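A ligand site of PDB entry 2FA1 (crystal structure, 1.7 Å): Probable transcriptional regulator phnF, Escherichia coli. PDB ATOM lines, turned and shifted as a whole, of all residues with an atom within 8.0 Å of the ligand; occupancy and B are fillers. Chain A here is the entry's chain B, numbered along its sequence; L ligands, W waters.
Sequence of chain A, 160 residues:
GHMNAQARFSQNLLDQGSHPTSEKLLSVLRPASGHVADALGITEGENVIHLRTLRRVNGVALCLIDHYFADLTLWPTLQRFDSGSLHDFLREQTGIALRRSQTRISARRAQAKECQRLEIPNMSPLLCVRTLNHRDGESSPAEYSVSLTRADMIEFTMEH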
ATOM      1  N   ARG A   8     -22.992  34.537  17.952  1.00  0.00           N
ATOM      2  CA  ARG A   8     -23.462  35.535  18.930  1.00  0.00           C
ATOM      3  C   ARG A   8     -22.341  36.210  19.704  1.00  0.00           C
ATOM      4  O   ARG A   8     -22.387  37.431  19.939  1.00  0.00           O
ATOM      5  CB  ARG A   8     -24.454  34.893  19.926  1.00  0.00           C
ATOM      6  CG  ARG A   8     -25.161  35.945  20.810  1.00  0.00           C
ATOM      7  CD  ARG A   8     -26.360  35.364  21.450  1.00  0.00           C
ATOM      8  NE  ARG A   8     -27.290  34.935  20.418  1.00  0.00           N
ATOM      9  CZ  ARG A   8     -28.208  33.995  20.518  1.00  0.00           C
ATOM     10  NH1 ARG A   8     -28.902  33.680  19.416  1.00  0.00           N
ATOM     11  NH2 ARG A   8     -28.463  33.377  21.666  1.00  0.00           N
ATOM     12  N   ARG A  56     -20.633  30.899  31.806  1.00  0.00           N
ATOM     13  CA  ARG A  56     -21.983  31.089  31.282  1.00  0.00           C
ATOM     14  C   ARG A  56     -22.161  32.531  30.863  1.00  0.00           C
ATOM     15  O   ARG A  56     -21.438  33.466  31.349  1.00  0.00           O
ATOM     16  CB  ARG A  56     -23.020  30.846  32.378  1.00  0.00           C
ATOM     17  CG  ARG A  56     -23.019  29.345  32.875  1.00  0.00           C
ATOM     18  CD  ARG A  56     -24.108  29.088  33.969  1.00  0.00           C
ATOM     19  NE  ARG A  56     -24.052  27.712  34.426  1.00  0.00           N
ATOM     20  CZ  ARG A  56     -24.754  26.705  33.918  1.00  0.00           C
ATOM     21  NH1 ARG A  56     -25.681  26.909  32.952  1.00  0.00           N
ATOM     22  NH2 ARG A  56     -24.568  25.464  34.366  1.00  0.00           N
ATOM     23  N   VAL A  57     -23.076  32.717  29.904  1.00  0.00           N
ATOM     24  CA  VAL A  57     -23.512  34.090  29.608  1.00  0.00           C
ATOM     25  C   VAL A  57     -25.034  34.112  29.722  1.00  0.00           C
ATOM     26  O   VAL A  57     -25.727  33.313  29.100  1.00  0.00           O
ATOM     27  CB  VAL A  57     -23.103  34.614  28.213  1.00  0.00           C
ATOM     28  CG1 VAL A  57     -23.595  36.079  28.081  1.00  0.00           C
ATOM     29  CG2 VAL A  57     -21.613  34.574  28.129  1.00  0.00           C
ATOM     30  N   ASN A  58     -25.484  34.978  30.606  1.00  0.00           N
ATOM     31  CA  ASN A  58     -26.945  35.075  30.925  1.00  0.00           C
ATOM     32  C   ASN A  58     -27.515  33.705  31.261  1.00  0.00           C
ATOM     33  O   ASN A  58     -28.582  33.327  30.766  1.00  0.00           O
ATOM     34  CB  ASN A  58     -27.707  35.692  29.714  1.00  0.00           C
ATOM     35  CG  ASN A  58     -27.447  37.102  29.546  1.00  0.00           C
ATOM     36  OD1 ASN A  58     -27.441  37.815  30.495  1.00  0.00           O
ATOM     37  ND2 ASN A  58     -27.232  37.545  28.260  1.00  0.00           N
ATOM     38  N   GLY A  59     -26.775  32.911  32.042  1.00  0.00           N
ATOM     39  CA  GLY A  59     -27.293  31.581  32.405  1.00  0.00           C
ATOM     40  C   GLY A  59     -26.875  30.369  31.527  1.00  0.00           C
ATOM     41  O   GLY A  59     -26.978  29.210  31.965  1.00  0.00           O
ATOM     42  N   VAL A  60     -26.442  30.673  30.307  1.00  0.00           N
ATOM     43  CA  VAL A  60     -26.276  29.666  29.296  1.00  0.00           C
ATOM     44  C   VAL A  60     -24.851  29.196  29.359  1.00  0.00           C
ATOM     45  O   VAL A  60     -23.946  30.005  29.138  1.00  0.00           O
ATOM     46  CB  VAL A  60     -26.580  30.234  27.862  1.00  0.00           C
ATOM     47  CG1 VAL A  60     -26.384  29.091  26.836  1.00  0.00           C
ATOM     48  CG2 VAL A  60     -28.092  30.751  27.859  1.00  0.00           C
ATOM     49  N   ALA A  61     -24.655  27.925  29.639  1.00  0.00           N
ATOM     50  CA  ALA A  61     -23.274  27.389  29.616  1.00  0.00           C
ATOM     51  C   ALA A  61     -22.661  27.447  28.197  1.00  0.00           C
ATOM     52  O   ALA A  61     -23.256  26.907  27.242  1.00  0.00           O
ATOM     53  CB  ALA A  61     -23.309  25.889  30.101  1.00  0.00           C
ATOM     54  N   LEU A  62     -21.440  27.996  28.066  1.00  0.00           N
ATOM     55  CA  LEU A  62     -20.858  28.231  26.762  1.00  0.00           C
ATOM     56  C   LEU A  62     -19.518  27.553  26.606  1.00  0.00           C
ATOM     57  O   LEU A  62     -19.216  27.081  25.514  1.00  0.00           O
ATOM     58  CB  LEU A  62     -20.598  29.751  26.509  1.00  0.00           C
ATOM     59  CG  LEU A  62     -21.791  30.735  26.517  1.00  0.00           C
ATOM     60  CD1 LEU A  62     -21.284  32.106  26.065  1.00  0.00           C
ATOM     61  CD2 LEU A  62     -22.910  30.317  25.607  1.00  0.00           C
ATOM     62  N   CYS A 115     -22.335  16.610  26.464  1.00  0.00           N
ATOM     63  CA  CYS A 115     -23.686  17.175  26.322  1.00  0.00           C
ATOM     64  C   CYS A 115     -24.236  17.544  27.664  1.00  0.00           C
ATOM     65  O   CYS A 115     -24.896  18.556  27.815  1.00  0.00           O
ATOM     66  CB  CYS A 115     -24.695  16.167  25.761  1.00  0.00           C
ATOM     67  SG  CYS A 115     -24.282  15.694  24.194  1.00  0.00           S
ATOM     68  N   LEU A 118     -22.126  20.625  29.305  1.00  0.00           N
ATOM     69  CA  LEU A 118     -22.323  21.862  28.530  1.00  0.00           C
ATOM     70  C   LEU A 118     -23.833  22.129  28.342  1.00  0.00           C
ATOM     71  O   LEU A 118     -24.232  23.193  27.799  1.00  0.00           O
ATOM     72  CB  LEU A 118     -21.621  21.751  27.229  1.00  0.00           C
ATOM     73  CG  LEU A 118     -20.292  22.487  27.181  1.00  0.00           C
ATOM     74  CD1 LEU A 118     -19.738  22.382  25.783  1.00  0.00           C
ATOM     75  CD2 LEU A 118     -20.346  23.999  27.542  1.00  0.00           C
ATOM     76  N   GLU A 119     -24.659  21.191  28.814  1.00  0.00           N
ATOM     77  CA  GLU A 119     -26.145  21.389  28.799  1.00  0.00           C
ATOM     78  C   GLU A 119     -26.692  21.601  27.379  1.00  0.00           C
ATOM     79  O   GLU A 119     -27.431  22.616  27.081  1.00  0.00           O
ATOM     80  CB  GLU A 119     -26.628  22.495  29.755  1.00  0.00           C
ATOM     81  CG  GLU A 119     -26.304  22.171  31.240  1.00  0.00           C
ATOM     82  CD  GLU A 119     -26.340  23.353  32.161  1.00  0.00           C
ATOM     83  OE1 GLU A 119     -26.672  24.524  31.750  1.00  0.00           O
ATOM     84  OE2 GLU A 119     -25.997  23.146  33.348  1.00  0.00           O
ATOM     85  N   ILE A 120     -26.307  20.703  26.497  1.00  0.00           N
ATOM     86  CA  ILE A 120     -26.663  20.804  25.049  1.00  0.00           C
ATOM     87  C   ILE A 120     -27.104  19.454  24.534  1.00  0.00           C
ATOM     88  O   ILE A 120     -26.745  18.411  25.132  1.00  0.00           O
ATOM     89  CB  ILE A 120     -25.454  21.347  24.218  1.00  0.00           C
ATOM     90  CG1 ILE A 120     -24.221  20.385  24.405  1.00  0.00           C
ATOM     91  CG2 ILE A 120     -25.155  22.806  24.659  1.00  0.00           C
ATOM     92  CD1 ILE A 120     -23.059  20.765  23.647  1.00  0.00           C
ATOM     93  N   PRO A 121     -27.928  19.457  23.453  1.00  0.00           N
ATOM     94  CA  PRO A 121     -28.486  18.231  22.925  1.00  0.00           C
ATOM     95  C   PRO A 121     -27.368  17.382  22.358  1.00  0.00           C
ATOM     96  O   PRO A 121     -26.316  17.904  21.943  1.00  0.00           O
ATOM     97  CB  PRO A 121     -29.424  18.683  21.806  1.00  0.00           C
ATOM     98  CG  PRO A 121     -29.703  20.221  22.113  1.00  0.00           C
ATOM     99  CD  PRO A 121     -28.365  20.651  22.700  1.00  0.00           C
ATOM    100  N   SER A 124     -24.626  18.193  19.188  1.00  0.00           N
ATOM    101  CA  SER A 124     -24.527  19.644  18.919  1.00  0.00           C
ATOM    102  C   SER A 124     -23.022  19.848  18.633  1.00  0.00           C
ATOM    103  O   SER A 124     -22.213  19.200  19.299  1.00  0.00           O
ATOM    104  CB  SER A 124     -24.948  20.399  20.201  1.00  0.00           C
ATOM    105  OG  SER A 124     -25.335  21.753  19.981  1.00  0.00           O
ATOM    106  N   ARG A 150     -19.573  25.762  22.869  1.00  0.00           N
ATOM    107  CA  ARG A 150     -20.659  25.628  21.938  1.00  0.00           C
ATOM    108  C   ARG A 150     -20.376  26.434  20.660  1.00  0.00           C
ATOM    109  O   ARG A 150     -20.339  27.630  20.665  1.00  0.00           O
ATOM    110  CB  ARG A 150     -21.943  26.165  22.643  1.00  0.00           C
ATOM    111  CG  ARG A 150     -22.465  25.242  23.629  1.00  0.00           C
ATOM    112  CD  ARG A 150     -23.782  25.812  24.205  1.00  0.00           C
ATOM    113  NE  ARG A 150     -24.757  26.021  23.104  1.00  0.00           N
ATOM    114  CZ  ARG A 150     -26.051  26.239  23.354  1.00  0.00           C
ATOM    115  NH1 ARG A 150     -26.481  26.248  24.639  1.00  0.00           N
ATOM    116  NH2 ARG A 150     -26.934  26.355  22.324  1.00  0.00           N
ATOM    117  N   ASP A 152     -22.301  26.811  18.198  1.00  0.00           N
ATOM    118  CA  ASP A 152     -23.430  27.667  17.737  1.00  0.00           C
ATOM    119  C   ASP A 152     -23.470  29.016  18.408  1.00  0.00           C
ATOM    120  O   ASP A 152     -24.331  29.853  18.013  1.00  0.00           O
ATOM    121  CB  ASP A 152     -24.797  26.959  17.921  1.00  0.00           C
ATOM    122  CG  ASP A 152     -25.148  26.754  19.344  1.00  0.00           C
ATOM    123  OD1 ASP A 152     -24.242  26.689  20.219  1.00  0.00           O
ATOM    124  OD2 ASP A 152     -26.346  26.458  19.592  1.00  0.00           O
ATOM    125  N   MET A 153     -22.615  29.289  19.445  1.00  0.00           N
ATOM    126  CA  MET A 153     -22.635  30.509  20.172  1.00  0.00           C
ATOM    127  C   MET A 153     -21.376  31.343  20.107  1.00  0.00           C
ATOM    128  O   MET A 153     -21.441  32.551  20.295  1.00  0.00           O
ATOM    129  CB  MET A 153     -22.942  30.300  21.644  1.00  0.00           C
ATOM    130  CG  MET A 153     -24.315  29.627  21.731  1.00  0.00           C
ATOM    131  SD  MET A 153     -25.563  30.968  21.804  1.00  0.00           S
ATOM    132  CE  MET A 153     -25.248  31.300  23.443  1.00  0.00           C
HETATM  133  C1  LIG L   1     -29.585  24.739  26.581  1.00  0.00           C
HETATM  134  C2  LIG L   1     -30.157  25.996  25.928  1.00  0.00           C
HETATM  135  C3  LIG L   1     -31.132  25.518  24.811  1.00  0.00           C
HETATM  136  C4  LIG L   1     -31.713  26.762  24.076  1.00  0.00           C
HETATM  137  C5  LIG L   1     -30.511  27.621  23.677  1.00  0.00           C
HETATM  138  C6  LIG L   1     -29.568  28.092  24.788  1.00  0.00           C
HETATM  139  O1  LIG L   1     -28.789  24.091  25.583  1.00  0.00           O
HETATM  140  O2  LIG L   1     -30.808  26.691  26.971  1.00  0.00           O
HETATM  141  O3  LIG L   1     -32.139  24.658  25.422  1.00  0.00           O
HETATM  142  O4  LIG L   1     -32.250  26.178  22.900  1.00  0.00           O
HETATM  143  O5  LIG L   1     -29.747  26.997  22.571  1.00  0.00           O
HETATM  144  O6  LIG L   1     -29.135  26.821  25.364  1.00  0.00           O
HETATM  145  O   HOH W   1     -33.330  25.903  27.503  1.00  0.00           O
HETATM  146  O   HOH W   2     -32.009  23.603  22.401  1.00  0.00           O
HETATM  147  O   HOH W   3     -29.261  27.492  28.916  1.00  0.00           O
HETATM  148  O   HOH W   4     -30.912  26.738  20.232  1.00  0.00           O
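Residues that only touch the ligand: Val 60 and Ile 120.
Hydrophobic or aromatic side chains within 4 Å of the ligand: Val 60 and Ile 120.
Within 4 Å of the ligand: Val 60, Glu 119, Ile 120 and Arg 150.
Along chain A the residues within 4 Å of the ligand span positions 60 to 150.
The nearest printed residue that does not touch the ligand is Pro 121 (4.5 Å).
The guanidinium group of Arg 150 lies within salt-bridge range of the side-chain carboxylate of Asp 152 (2.8 Å).
O of Cys 115 is in hydrogen-bond range of N of Ile 120 (2.9 Å).
The backbone NH of Arg 150 sits at hydrogen-bond distance from the backbone carbonyl oxygen of Leu 62 (3.0 Å).
The side-chain carboxylate (OE1) of Glu 119 lies within salt-bridge range of the guanidinium group (NH1) of Arg 56, 2.8 Å away.
An oxygen (O6) of the ligand is in hydrogen-bond range of the guanidinium group (NH1) of Arg 150 (2.8 Å).
An oxygen (O1) of the ligand lies within hydrogen-bond range of the backbone carbonyl oxygen (O) of Glu 119 (2.5 Å).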
